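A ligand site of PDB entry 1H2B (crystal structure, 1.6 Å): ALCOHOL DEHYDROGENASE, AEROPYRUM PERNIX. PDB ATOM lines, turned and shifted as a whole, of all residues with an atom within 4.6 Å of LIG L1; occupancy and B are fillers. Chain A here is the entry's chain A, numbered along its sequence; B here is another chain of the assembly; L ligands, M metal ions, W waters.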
ATOM      1  N   CYS A  54       6.499  32.223  25.164  1.00  0.00           N
ATOM      2  CA  CYS A  54       7.880  31.873  25.424  1.00  0.00           C
ATOM      3  C   CYS A  54       8.263  32.196  26.874  1.00  0.00           C
ATOM      4  O   CYS A  54       7.690  33.099  27.470  1.00  0.00           O
ATOM      5  CB  CYS A  54       8.765  32.701  24.473  1.00  0.00           C
ATOM      6  SG  CYS A  54      10.537  32.389  24.550  1.00  0.00           S
ATOM      7  N   HIS A  55       9.235  31.514  27.444  1.00  0.00           N
ATOM      8  CA  HIS A  55       9.684  31.907  28.774  1.00  0.00           C
ATOM      9  C   HIS A  55      10.226  33.351  28.756  1.00  0.00           C
ATOM     10  O   HIS A  55      10.196  34.024  29.774  1.00  0.00           O
ATOM     11  CB  HIS A  55      10.683  30.936  29.339  1.00  0.00           C
ATOM     12  CG  HIS A  55      10.756  30.927  30.837  1.00  0.00           C
ATOM     13  ND1 HIS A  55      10.494  29.788  31.579  1.00  0.00           N
ATOM     14  CD2 HIS A  55      11.078  31.892  31.731  1.00  0.00           C
ATOM     15  CE1 HIS A  55      10.669  30.062  32.872  1.00  0.00           C
ATOM     16  NE2 HIS A  55      11.035  31.325  32.991  1.00  0.00           N
ATOM     17  N   THR A  56      10.672  33.838  27.611  1.00  0.00           N
ATOM     18  CA  THR A  56      11.097  35.244  27.500  1.00  0.00           C
ATOM     19  C   THR A  56       9.965  36.179  27.875  1.00  0.00           C
ATOM     20  O   THR A  56      10.230  37.284  28.393  1.00  0.00           O
ATOM     21  CB  THR A  56      11.603  35.509  26.076  1.00  0.00           C
ATOM     22  OG1 THR A  56      12.908  34.933  25.961  1.00  0.00           O
ATOM     23  CG2 THR A  56      11.772  37.021  25.780  1.00  0.00           C
ATOM     24  N   HIS A  59      10.115  36.712  31.447  1.00  0.00           N
ATOM     25  CA  HIS A  59      11.216  37.613  31.734  1.00  0.00           C
ATOM     26  C   HIS A  59      10.838  39.044  31.397  1.00  0.00           C
ATOM     27  O   HIS A  59      11.232  39.989  32.117  1.00  0.00           O
ATOM     28  CB  HIS A  59      12.438  37.218  30.894  1.00  0.00           C
ATOM     29  CG  HIS A  59      13.045  35.887  31.226  1.00  0.00           C
ATOM     30  ND1 HIS A  59      13.050  35.330  32.501  1.00  0.00           N
ATOM     31  CD2 HIS A  59      13.707  35.004  30.424  1.00  0.00           C
ATOM     32  CE1 HIS A  59      13.683  34.174  32.458  1.00  0.00           C
ATOM     33  NE2 HIS A  59      14.092  33.948  31.214  1.00  0.00           N
ATOM     34  N   ASP A 168      10.417  30.791  16.953  1.00  0.00           N
ATOM     35  CA  ASP A 168      11.327  31.297  17.960  1.00  0.00           C
ATOM     36  C   ASP A 168      11.941  30.154  18.752  1.00  0.00           C
ATOM     37  O   ASP A 168      13.154  29.970  18.748  1.00  0.00           O
ATOM     38  CB  ASP A 168      10.582  32.315  18.862  1.00  0.00           C
ATOM     39  CG  ASP A 168      11.488  32.935  19.862  1.00  0.00           C
ATOM     40  OD1 ASP A 168      11.328  32.644  21.053  1.00  0.00           O
ATOM     41  OD2 ASP A 168      12.437  33.683  19.546  1.00  0.00           O
ATOM     42  N   THR A 172      15.646  28.932  17.469  1.00  0.00           N
ATOM     43  CA  THR A 172      16.713  29.104  18.474  1.00  0.00           C
ATOM     44  C   THR A 172      17.372  27.765  18.795  1.00  0.00           C
ATOM     45  O   THR A 172      18.605  27.659  18.810  1.00  0.00           O
ATOM     46  CB  THR A 172      16.154  29.704  19.750  1.00  0.00           C
ATOM     47  OG1 THR A 172      15.580  30.963  19.437  1.00  0.00           O
ATOM     48  CG2 THR A 172      17.267  29.976  20.750  1.00  0.00           C
ATOM     49  N   VAL A 193      19.932  20.536  28.504  1.00  0.00           N
ATOM     50  CA  VAL A 193      19.497  20.841  29.856  1.00  0.00           C
ATOM     51  C   VAL A 193      18.259  21.692  29.730  1.00  0.00           C
ATOM     52  O   VAL A 193      18.306  22.845  29.225  1.00  0.00           O
ATOM     53  CB  VAL A 193      20.630  21.583  30.650  1.00  0.00           C
ATOM     54  CG1 VAL A 193      20.143  21.928  32.077  1.00  0.00           C
ATOM     55  CG2 VAL A 193      21.864  20.698  30.734  1.00  0.00           C
ATOM     56  N   GLY A 194      17.131  21.122  30.182  1.00  0.00           N
ATOM     57  CA  GLY A 194      15.864  21.841  30.127  1.00  0.00           C
ATOM     58  C   GLY A 194      15.056  21.367  28.956  1.00  0.00           C
ATOM     59  O   GLY A 194      15.244  21.869  27.838  1.00  0.00           O
ATOM     60  N   VAL A 195      14.132  20.436  29.199  1.00  0.00           N
ATOM     61  CA  VAL A 195      13.320  19.898  28.092  1.00  0.00           C
ATOM     62  C   VAL A 195      11.997  20.717  28.036  1.00  0.00           C
ATOM     63  O   VAL A 195      10.869  20.220  28.283  1.00  0.00           O
ATOM     64  CB  VAL A 195      13.054  18.404  28.311  1.00  0.00           C
ATOM     65  CG1 VAL A 195      12.330  17.813  27.098  1.00  0.00           C
ATOM     66  CG2 VAL A 195      14.394  17.679  28.637  1.00  0.00           C
ATOM     67  N   GLY A 196      12.162  22.001  27.753  1.00  0.00           N
ATOM     68  CA  GLY A 196      11.039  22.919  27.741  1.00  0.00           C
ATOM     69  C   GLY A 196      10.594  23.234  26.356  1.00  0.00           C
ATOM     70  O   GLY A 196      10.681  22.383  25.427  1.00  0.00           O
ATOM     71  N   GLY A 197      10.067  24.442  26.164  1.00  0.00           N
ATOM     72  CA  GLY A 197       9.602  24.815  24.853  1.00  0.00           C
ATOM     73  C   GLY A 197      10.709  24.712  23.833  1.00  0.00           C
ATOM     74  O   GLY A 197      10.530  24.065  22.792  1.00  0.00           O
ATOM     75  N   LEU A 198      11.854  25.317  24.130  1.00  0.00           N
ATOM     76  CA  LEU A 198      13.015  25.134  23.242  1.00  0.00           C
ATOM     77  C   LEU A 198      13.658  23.775  23.364  1.00  0.00           C
ATOM     78  O   LEU A 198      13.977  23.143  22.337  1.00  0.00           O
ATOM     79  CB  LEU A 198      14.106  26.161  23.560  1.00  0.00           C
ATOM     80  CG  LEU A 198      13.948  27.547  22.954  1.00  0.00           C
ATOM     81  CD1 LEU A 198      12.727  28.313  23.499  1.00  0.00           C
ATOM     82  CD2 LEU A 198      15.277  28.277  23.176  1.00  0.00           C
ATOM     83  N   GLY A 199      13.850  23.309  24.587  1.00  0.00           N
ATOM     84  CA  GLY A 199      14.670  22.128  24.796  1.00  0.00           C
ATOM     85  C   GLY A 199      14.048  20.863  24.187  1.00  0.00           C
ATOM     86  O   GLY A 199      14.811  20.032  23.684  1.00  0.00           O
ATOM     87  N   LEU A 217      18.275  16.606  30.619  1.00  0.00           N
ATOM     88  CA  LEU A 217      18.163  16.911  32.046  1.00  0.00           C
ATOM     89  C   LEU A 217      16.944  17.798  32.274  1.00  0.00           C
ATOM     90  O   LEU A 217      16.631  18.680  31.490  1.00  0.00           O
ATOM     91  CB  LEU A 217      19.418  17.656  32.561  1.00  0.00           C
ATOM     92  CG  LEU A 217      20.596  16.845  33.026  1.00  0.00           C
ATOM     93  CD1 LEU A 217      21.187  16.164  31.836  1.00  0.00           C
ATOM     94  CD2 LEU A 217      21.657  17.824  33.612  1.00  0.00           C
ATOM     95  N   ASP A 218      16.160  17.446  33.297  1.00  0.00           N
ATOM     96  CA  ASP A 218      15.053  18.332  33.693  1.00  0.00           C
ATOM     97  C   ASP A 218      14.732  17.978  35.134  1.00  0.00           C
ATOM     98  O   ASP A 218      15.443  17.187  35.772  1.00  0.00           O
ATOM     99  CB  ASP A 218      13.829  18.194  32.778  1.00  0.00           C
ATOM    100  CG  ASP A 218      12.990  19.460  32.697  1.00  0.00           C
ATOM    101  OD1 ASP A 218      12.851  20.024  31.600  1.00  0.00           O
ATOM    102  OD2 ASP A 218      12.351  19.896  33.695  1.00  0.00           O
ATOM    103  N   VAL A 219      13.672  18.601  35.647  1.00  0.00           N
ATOM    104  CA  VAL A 219      13.346  18.533  37.089  1.00  0.00           C
ATOM    105  C   VAL A 219      11.877  18.254  37.312  1.00  0.00           C
ATOM    106  O   VAL A 219      11.359  18.462  38.427  1.00  0.00           O
ATOM    107  CB  VAL A 219      13.723  19.872  37.782  1.00  0.00           C
ATOM    108  CG1 VAL A 219      15.255  20.136  37.766  1.00  0.00           C
ATOM    109  CG2 VAL A 219      12.970  21.070  37.151  1.00  0.00           C
ATOM    110  N   LYS A 220      11.170  17.809  36.266  1.00  0.00           N
ATOM    111  CA  LYS A 220       9.796  17.299  36.358  1.00  0.00           C
ATOM    112  C   LYS A 220       9.711  15.982  35.631  1.00  0.00           C
ATOM    113  O   LYS A 220      10.110  15.879  34.472  1.00  0.00           O
ATOM    114  CB  LYS A 220       8.762  18.220  35.687  1.00  0.00           C
ATOM    115  CG  LYS A 220       8.784  19.673  36.123  1.00  0.00           C
ATOM    116  CD  LYS A 220       8.109  19.869  37.483  1.00  0.00           C
ATOM    117  CE  LYS A 220       7.657  21.320  37.617  1.00  0.00           C
ATOM    118  NZ  LYS A 220       6.860  21.570  38.875  1.00  0.00           N
ATOM    119  N   LYS A 223       8.520  15.688  32.031  1.00  0.00           N
ATOM    120  CA  LYS A 223       9.391  16.287  30.983  1.00  0.00           C
ATOM    121  C   LYS A 223      10.530  15.323  30.618  1.00  0.00           C
ATOM    122  O   LYS A 223      10.956  15.294  29.439  1.00  0.00           O
ATOM    123  CB  LYS A 223       9.898  17.657  31.421  1.00  0.00           C
ATOM    124  CG  LYS A 223       8.723  18.624  31.650  1.00  0.00           C
ATOM    125  CD  LYS A 223       9.223  19.943  32.222  1.00  0.00           C
ATOM    126  CE  LYS A 223       8.138  20.900  32.683  1.00  0.00           C
ATOM    127  NZ  LYS A 223       7.139  21.209  31.656  1.00  0.00           N
ATOM    128  N   ALA A 238      17.689  16.499  37.388  1.00  0.00           N
ATOM    129  CA  ALA A 238      18.716  17.427  37.867  1.00  0.00           C
ATOM    130  C   ALA A 238      18.473  17.931  39.281  1.00  0.00           C
ATOM    131  O   ALA A 238      19.225  18.773  39.797  1.00  0.00           O
ATOM    132  CB  ALA A 238      18.892  18.592  36.878  1.00  0.00           C
ATOM    133  N   PHE A 261      19.213  25.211  28.010  1.00  0.00           N
ATOM    134  CA  PHE A 261      17.940  25.748  27.545  1.00  0.00           C
ATOM    135  C   PHE A 261      17.022  26.122  28.719  1.00  0.00           C
ATOM    136  O   PHE A 261      15.809  26.066  28.601  1.00  0.00           O
ATOM    137  CB  PHE A 261      17.218  24.697  26.645  1.00  0.00           C
ATOM    138  CG  PHE A 261      17.849  24.551  25.261  1.00  0.00           C
ATOM    139  CD1 PHE A 261      18.682  23.454  24.975  1.00  0.00           C
ATOM    140  CD2 PHE A 261      17.568  25.487  24.262  1.00  0.00           C
ATOM    141  CE1 PHE A 261      19.282  23.293  23.699  1.00  0.00           C
ATOM    142  CE2 PHE A 261      18.111  25.338  22.972  1.00  0.00           C
ATOM    143  CZ  PHE A 261      18.995  24.258  22.689  1.00  0.00           C
ATOM    144  N   VAL A 262      17.652  26.500  29.829  1.00  0.00           N
ATOM    145  CA  VAL A 262      16.920  26.964  31.015  1.00  0.00           C
ATOM    146  C   VAL A 262      17.367  28.392  31.348  1.00  0.00           C
ATOM    147  O   VAL A 262      16.525  29.318  31.359  1.00  0.00           O
ATOM    148  CB  VAL A 262      17.199  26.088  32.207  1.00  0.00           C
ATOM    149  CG1 VAL A 262      16.290  26.534  33.412  1.00  0.00           C
ATOM    150  CG2 VAL A 262      16.933  24.632  31.880  1.00  0.00           C
ATOM    151  N   GLY A 263      18.652  28.553  31.657  1.00  0.00           N
ATOM    152  CA  GLY A 263      19.223  29.863  31.890  1.00  0.00           C
ATOM    153  C   GLY A 263      19.058  30.354  33.321  1.00  0.00           C
ATOM    154  O   GLY A 263      19.428  31.479  33.605  1.00  0.00           O
ATOM    155  N   ALA A 266      20.499  28.311  38.884  1.00  0.00           N
ATOM    156  CA  ALA A 266      20.728  26.882  39.143  1.00  0.00           C
ATOM    157  C   ALA A 266      21.453  26.187  37.990  1.00  0.00           C
ATOM    158  O   ALA A 266      22.484  25.494  38.179  1.00  0.00           O
ATOM    159  CB  ALA A 266      19.370  26.201  39.433  1.00  0.00           C
ATOM    160  N   THR A 267      20.940  26.387  36.782  1.00  0.00           N
ATOM    161  CA  THR A 267      21.553  25.634  35.673  1.00  0.00           C
ATOM    162  C   THR A 267      22.873  26.242  35.240  1.00  0.00           C
ATOM    163  O   THR A 267      23.814  25.534  34.853  1.00  0.00           O
ATOM    164  CB  THR A 267      20.625  25.505  34.420  1.00  0.00           C
ATOM    165  OG1 THR A 267      20.225  26.777  33.940  1.00  0.00           O
ATOM    166  CG2 THR A 267      19.321  24.862  34.814  1.00  0.00           C
ATOM    167  N   TYR A 270      25.606  24.771  37.379  1.00  0.00           N
ATOM    168  CA  TYR A 270      26.115  23.407  37.236  1.00  0.00           C
ATOM    169  C   TYR A 270      26.514  23.028  35.838  1.00  0.00           C
ATOM    170  O   TYR A 270      27.378  22.154  35.665  1.00  0.00           O
ATOM    171  CB  TYR A 270      25.168  22.330  37.844  1.00  0.00           C
ATOM    172  CG  TYR A 270      23.864  21.988  37.091  1.00  0.00           C
ATOM    173  CD1 TYR A 270      23.877  21.204  35.914  1.00  0.00           C
ATOM    174  CD2 TYR A 270      22.635  22.388  37.575  1.00  0.00           C
ATOM    175  CE1 TYR A 270      22.720  20.873  35.246  1.00  0.00           C
ATOM    176  CE2 TYR A 270      21.427  22.054  36.911  1.00  0.00           C
ATOM    177  CZ  TYR A 270      21.499  21.289  35.748  1.00  0.00           C
ATOM    178  OH  TYR A 270      20.324  20.965  35.128  1.00  0.00           O
ATOM    179  N   VAL A 284      21.836  29.200  25.907  1.00  0.00           N
ATOM    180  CA  VAL A 284      20.634  29.638  25.252  1.00  0.00           C
ATOM    181  C   VAL A 284      19.688  30.316  26.213  1.00  0.00           C
ATOM    182  O   VAL A 284      19.282  31.455  26.011  1.00  0.00           O
ATOM    183  CB  VAL A 284      19.920  28.474  24.498  1.00  0.00           C
ATOM    184  CG1 VAL A 284      18.719  29.008  23.747  1.00  0.00           C
ATOM    185  CG2 VAL A 284      20.930  27.805  23.522  1.00  0.00           C
ATOM    186  N   GLY A 285      19.344  29.611  27.299  1.00  0.00           N
ATOM    187  CA  GLY A 285      18.542  30.266  28.303  1.00  0.00           C
ATOM    188  C   GLY A 285      19.347  31.367  28.987  1.00  0.00           C
ATOM    189  O   GLY A 285      20.572  31.388  28.969  1.00  0.00           O
ATOM    190  N   TYR A 286      18.613  32.318  29.583  1.00  0.00           N
ATOM    191  CA  TYR A 286      19.331  33.381  30.286  1.00  0.00           C
ATOM    192  C   TYR A 286      18.548  33.790  31.514  1.00  0.00           C
ATOM    193  O   TYR A 286      17.414  33.416  31.717  1.00  0.00           O
ATOM    194  CB  TYR A 286      19.562  34.575  29.339  1.00  0.00           C
ATOM    195  CG  TYR A 286      18.257  35.133  28.830  1.00  0.00           C
ATOM    196  CD1 TYR A 286      17.571  36.129  29.515  1.00  0.00           C
ATOM    197  CD2 TYR A 286      17.684  34.633  27.653  1.00  0.00           C
ATOM    198  CE1 TYR A 286      16.347  36.607  29.046  1.00  0.00           C
ATOM    199  CE2 TYR A 286      16.450  35.098  27.176  1.00  0.00           C
ATOM    200  CZ  TYR A 286      15.787  36.083  27.901  1.00  0.00           C
ATOM    201  OH  TYR A 286      14.580  36.515  27.492  1.00  0.00           O
ATOM    202  N   SER A 307      24.107  31.666  22.034  1.00  0.00           N
ATOM    203  CA  SER A 307      23.379  31.487  20.789  1.00  0.00           C
ATOM    204  C   SER A 307      22.123  32.308  20.862  1.00  0.00           C
ATOM    205  O   SER A 307      21.428  32.294  21.883  1.00  0.00           O
ATOM    206  CB  SER A 307      23.102  29.980  20.563  1.00  0.00           C
ATOM    207  OG  SER A 307      22.791  29.757  19.188  1.00  0.00           O
ATOM    208  N   LEU A 308      21.838  33.015  19.768  1.00  0.00           N
ATOM    209  CA  LEU A 308      20.770  33.987  19.747  1.00  0.00           C
ATOM    210  C   LEU A 308      19.808  33.735  18.593  1.00  0.00           C
ATOM    211  O   LEU A 308      20.165  33.935  17.412  1.00  0.00           O
ATOM    212  CB  LEU A 308      21.385  35.399  19.654  1.00  0.00           C
ATOM    213  CG  LEU A 308      20.386  36.556  19.476  1.00  0.00           C
ATOM    214  CD1 LEU A 308      19.505  36.719  20.727  1.00  0.00           C
ATOM    215  CD2 LEU A 308      21.119  37.874  19.158  1.00  0.00           C
ATOM    216  N   VAL A 309      18.584  33.310  18.938  1.00  0.00           N
ATOM    217  CA  VAL A 309      17.534  33.086  17.942  1.00  0.00           C
ATOM    218  C   VAL A 309      18.148  32.394  16.728  1.00  0.00           C
ATOM    219  O   VAL A 309      18.771  31.344  16.882  1.00  0.00           O
ATOM    220  CB  VAL A 309      16.671  34.365  17.661  1.00  0.00           C
ATOM    221  CG1 VAL A 309      15.344  34.014  16.971  1.00  0.00           C
ATOM    222  CG2 VAL A 309      16.342  35.118  18.998  1.00  0.00           C
ATOM    223  N   LEU A 346       3.349  28.466  32.961  1.00  0.00           N
ATOM    224  CA  LEU A 346       4.713  28.364  32.431  1.00  0.00           C
ATOM    225  C   LEU A 346       5.717  28.693  33.544  1.00  0.00           C
ATOM    226  O   LEU A 346       6.721  28.030  33.718  1.00  0.00           O
ATOM    227  CB  LEU A 346       4.891  29.273  31.197  1.00  0.00           C
ATOM    228  CG  LEU A 346       6.238  29.117  30.458  1.00  0.00           C
ATOM    229  CD1 LEU A 346       6.392  27.718  29.851  1.00  0.00           C
ATOM    230  CD2 LEU A 346       6.278  30.198  29.357  1.00  0.00           C
ATOM    231  N   GLY A 353       5.927  21.016  26.803  1.00  0.00           N
ATOM    232  CA  GLY A 353       6.341  21.532  25.505  1.00  0.00           C
ATOM    233  C   GLY A 353       6.042  23.012  25.420  1.00  0.00           C
ATOM    234  O   GLY A 353       6.544  23.767  26.276  1.00  0.00           O
ATOM    235  N   ARG A 354       5.246  23.404  24.421  1.00  0.00           N
ATOM    236  CA  ARG A 354       5.005  24.818  24.112  1.00  0.00           C
ATOM    237  C   ARG A 354       3.540  25.168  24.094  1.00  0.00           C
ATOM    238  O   ARG A 354       2.786  24.570  23.379  1.00  0.00           O
ATOM    239  CB  ARG A 354       5.589  25.139  22.725  1.00  0.00           C
ATOM    240  CG  ARG A 354       5.765  26.614  22.379  1.00  0.00           C
ATOM    241  CD  ARG A 354       6.490  27.413  23.417  1.00  0.00           C
ATOM    242  NE  ARG A 354       7.382  28.397  22.863  1.00  0.00           N
ATOM    243  CZ  ARG A 354       8.419  28.863  23.551  1.00  0.00           C
ATOM    244  NH1 ARG A 354       8.693  28.398  24.776  1.00  0.00           N
ATOM    245  NH2 ARG A 354       9.181  29.799  22.970  1.00  0.00           N
ATOM    246  N   ILE B 298      23.768  36.003  25.568  1.00  0.00           N
ATOM    247  CA  ILE B 298      22.883  35.716  24.428  1.00  0.00           C
ATOM    248  C   ILE B 298      22.562  36.981  23.622  1.00  0.00           C
ATOM    249  O   ILE B 298      22.520  36.909  22.380  1.00  0.00           O
ATOM    250  CB  ILE B 298      21.625  34.877  24.852  1.00  0.00           C
ATOM    251  CG1 ILE B 298      20.610  35.713  25.621  1.00  0.00           C
ATOM    252  CG2 ILE B 298      22.050  33.651  25.652  1.00  0.00           C
ATOM    253  CD1 ILE B 298      19.546  36.390  24.771  1.00  0.00           C
HETATM  254  P1  LIG L   1      10.445  26.710  29.397  1.00  0.00           P
HETATM  255  O1  LIG L   1       9.897  27.341  30.675  1.00  0.00           O
HETATM  256  O2  LIG L   1       9.441  26.101  28.431  1.00  0.00           O
HETATM  257  O3  LIG L   1      11.440  25.533  29.709  1.00  0.00           O
HETATM  258  C1  LIG L   1      12.399  25.564  30.765  1.00  0.00           C
HETATM  259  C2  LIG L   1      12.674  24.100  31.096  1.00  0.00           C
HETATM  260  O4  LIG L   1      13.696  24.066  32.067  1.00  0.00           O
HETATM  261  C3  LIG L   1      11.460  23.374  31.757  1.00  0.00           C
HETATM  262  O5  LIG L   1      11.168  22.167  31.076  1.00  0.00           O
HETATM  263  C4  LIG L   1      11.893  23.257  33.201  1.00  0.00           C
HETATM  264  O6  LIG L   1      11.268  22.223  33.955  1.00  0.00           O
HETATM  265  C5  LIG L   1      13.389  23.068  33.042  1.00  0.00           C
HETATM  266  N1  LIG L   1      14.128  23.364  34.261  1.00  0.00           N
HETATM  267  C6  LIG L   1      13.880  24.286  35.257  1.00  0.00           C
HETATM  268  N2  LIG L   1      14.883  24.209  36.153  1.00  0.00           N
HETATM  269  C7  LIG L   1      15.775  23.248  35.747  1.00  0.00           C
HETATM  270  C8  LIG L   1      16.943  22.724  36.286  1.00  0.00           C
HETATM  271  N3  LIG L   1      17.465  23.151  37.446  1.00  0.00           N
HETATM  272  N4  LIG L   1      17.641  21.737  35.600  1.00  0.00           N
HETATM  273  C9  LIG L   1      17.089  21.242  34.414  1.00  0.00           C
HETATM  274  N5  LIG L   1      15.946  21.726  33.893  1.00  0.00           N
HETATM  275  C10 LIG L   1      15.285  22.721  34.550  1.00  0.00           C
HETATM  276  O7  LIG L   1      11.317  27.868  28.718  1.00  0.00           O
HETATM  277  P2  LIG L   1      11.595  28.123  27.152  1.00  0.00           P
HETATM  278  O8  LIG L   1      10.512  28.966  26.617  1.00  0.00           O
HETATM  279  O9  LIG L   1      11.987  26.836  26.548  1.00  0.00           O
HETATM  280  O10 LIG L   1      12.887  29.052  27.291  1.00  0.00           O
HETATM  281  C11 LIG L   1      14.092  28.490  27.785  1.00  0.00           C
HETATM  282  C12 LIG L   1      15.139  29.580  28.086  1.00  0.00           C
HETATM  283  O11 LIG L   1      15.580  30.122  26.814  1.00  0.00           O
HETATM  284  C13 LIG L   1      14.549  30.808  28.805  1.00  0.00           C
HETATM  285  O12 LIG L   1      15.558  31.359  29.621  1.00  0.00           O
HETATM  286  C14 LIG L   1      14.158  31.752  27.689  1.00  0.00           C
HETATM  287  O13 LIG L   1      14.019  33.093  28.083  1.00  0.00           O
HETATM  288  C15 LIG L   1      15.369  31.528  26.790  1.00  0.00           C
HETATM  289  N6  LIG L   1      15.259  31.984  25.393  1.00  0.00           N
HETATM  290  C16 LIG L   1      16.452  32.230  24.772  1.00  0.00           C
HETATM  291  C17 LIG L   1      16.458  32.552  23.427  1.00  0.00           C
HETATM  292  C18 LIG L   1      17.782  32.894  22.786  1.00  0.00           C
HETATM  293  O14 LIG L   1      17.705  33.295  21.529  1.00  0.00           O
HETATM  294  N7  LIG L   1      18.932  32.807  23.432  1.00  0.00           N
HETATM  295  C19 LIG L   1      15.269  32.567  22.639  1.00  0.00           C
HETATM  296  C20 LIG L   1      14.074  32.137  23.278  1.00  0.00           C
HETATM  297  C21 LIG L   1      14.107  31.835  24.633  1.00  0.00           C
HETATM  298  C1  LG2 L   2      13.580  35.374  22.446  1.00  0.00           C
HETATM  299  C2  LG2 L   2      14.693  36.253  22.999  1.00  0.00           C
HETATM  300  C3  LG2 L   2      15.222  37.191  21.909  1.00  0.00           C
HETATM  301  C4  LG2 L   2      15.933  38.420  22.471  1.00  0.00           C
HETATM  302  C5  LG2 L   2      16.520  39.211  21.301  1.00  0.00           C
HETATM  303  C6  LG2 L   2      17.724  40.042  21.735  1.00  0.00           C
HETATM  304  C7  LG2 L   2      18.120  40.999  20.595  1.00  0.00           C
HETATM  305  C8  LG2 L   2      19.602  41.373  20.609  1.00  0.00           C
HETATM  306  O1  LG2 L   2      12.829  34.744  23.269  1.00  0.00           O
HETATM  307  O2  LG2 L   2      13.377  35.351  21.204  1.00  0.00           O
HETATM  308 ZN    ZN M   1      11.223  33.726  22.873  1.00  0.00          ZN
HETATM  309  O   HOH W   1       7.316  26.468  26.676  1.00  0.00           O
HETATM  310  O   HOH W   2      15.667  24.224  39.565  1.00  0.00           O
HETATM  311  O   HOH W   3      13.559  24.745  27.132  1.00  0.00           O
HETATM  312  O   HOH W   4       8.385  26.190  32.527  1.00  0.00           O
HETATM  313  O   HOH W   5       7.806  23.891  28.994  1.00  0.00           O
HETATM  314  O   HOH W   6      10.009  23.527  36.022  1.00  0.00           O
HETATM  315  O   HOH W   7      15.987  26.535  37.481  1.00  0.00           O
HETATM  316  O   HOH W   8      19.129  21.587  39.461  1.00  0.00           O
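Merely in contact with LIG L1: Phe 261 (3.1 Å), Lys 223 (3.2 Å), Gly 285 (3.3 Å), Val 219 (3.4 Å), Thr 172 (3.4 Å), Thr 267 (3.5 Å), Asp 168 (3.6 Å), Leu 308 (3.6 Å), Cys 54 (3.6 Å), Ala 238 (3.6 Å), Leu 346 (3.6 Å), Gly 194 (3.7 Å), Ile 298 of chain B (3.7 Å), Val 193 (3.9 Å) and Leu 217 (3.9 Å).
Hydrophobic or aromatic side chains within 4 Å of LIG L1: His 55, His 59, Val 193, Leu 198, Val 219, Ala 238, Val 262, Tyr 270, Val 284, Tyr 286, Leu 308, Val 309, Leu 346 and Ile 298 of chain B.
30 residues have an atom within 4 Å of LIG L1: Cys 54, His 55, Thr 56, His 59, Asp 168, Thr 172, Val 193, Gly 194, Val 195, Gly 196, Gly 197, Leu 198, Leu 217, Asp 218, Val 219, Lys 223, Ala 238, Phe 261, Val 262, Thr 267, Tyr 270, Val 284, Gly 285, Tyr 286, Ser 307, Leu 308, Val 309, Leu 346, Arg 354 and Ile 298 of chain B.
The side-chain carboxylate (OD1) of Asp 218 is in hydrogen-bond range of the backbone NH (N) of Val 195, at 2.8 Å.
SG of Cys 54 lies close to NH2 of Arg 354 (3.3 Å).
The side-chain hydroxyl (OG1) of Thr 56 lies within hydrogen-bond range of the side-chain hydroxyl (OH) of Tyr 286 (2.8 Å).
The side-chain sulfur of Cys 54 lies close to the backbone NH of Thr 56, 3.4 Å away.
A ring nitrogen (NE2) of His 59 lies within hydrogen-bond range of the backbone carbonyl oxygen of Tyr 286 (3.4 Å).
O of Val 193 sits at hydrogen-bond distance from N of Phe 261 (2.8 Å).
OG1 of Thr 267 sits at hydrogen-bond distance from N of Gly 263 (3.3 Å).
The backbone NH (N) of Gly 194 sits at hydrogen-bond distance from the backbone carbonyl oxygen (O) of Leu 217, 2.8 Å away.
OD2 of Asp 218 sits at hydrogen-bond distance from O6 of LIG L1, at 2.6 Å.
The guanidinium group of Arg 354 lies within salt-bridge range of an oxygen (O8) of LIG L1, at 2.6 Å.
The backbone NH (N) of His 55 lies within hydrogen-bond range of an oxygen (O8) of LIG L1.
A ring nitrogen (ND1) of His 55 lies within hydrogen-bond range of an oxygen (O1) of LIG L1 (2.7 Å).
The backbone NH of Val 309 lies within hydrogen-bond range of an oxygen (O14) of LIG L1.
The side-chain hydroxyl of Tyr 270 sits at hydrogen-bond distance from a nitrogen (N4) of LIG L1, at 2.8 Å.
O of Val 262 lies within hydrogen-bond range of O12 of LIG L1 (2.8 Å).
O9 of LIG L1 lies within hydrogen-bond range of N of Leu 198 (2.9 Å).
N of Gly 197 sits at hydrogen-bond distance from O2 of LIG L1 (2.9 Å).
The backbone carbonyl oxygen of Val 284 is in hydrogen-bond range of a nitrogen (N7) of LIG L1.
The backbone carbonyl oxygen (O) of Ser 307 sits at hydrogen-bond distance from a nitrogen (N7) of LIG L1, 3.0 Å away.
N of Thr 56 lies within hydrogen-bond range of O13 of LIG L1.
The side-chain hydroxyl (OG1) of Thr 56 lies within hydrogen-bond range of an oxygen (O13) of LIG L1 (3.0 Å).
A ring nitrogen (NE2) of His 59 sits close to an oxygen (O13) of LIG L1.
An oxygen (O12) of LIG L1 lies within hydrogen-bond range of the backbone NH (N) of Tyr 286.
O12 of LIG L1 is in hydrogen-bond range of O of Tyr 286, at 3.5 Å.
N of Gly 196 sits close to O5 of LIG L1, at 3.5 Å.
The backbone carbonyl oxygen of Val 195 is in hydrogen-bond range of an oxygen (O5) of LIG L1 (3.4 Å).
O1 of LG2 L2 sits close to OG1 of Thr 56, at 2.7 Å.
Water W4 bridges O1 of LIG L1 (2.7 Å) and O of Leu 346 (2.8 Å).
Water W1 lies within hydrogen-bond range of O2 of LIG L1 (2.8 Å), O of Gly 353 (2.8 Å), NH1 of Arg 354 (3.0 Å) and N of Gly 197 (3.5 Å).
Water W5 lies within hydrogen-bond range of O2 of LIG L1 and O of Gly 353.
Water W8 bridges O of Ala 238 and N3 of LIG L1.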
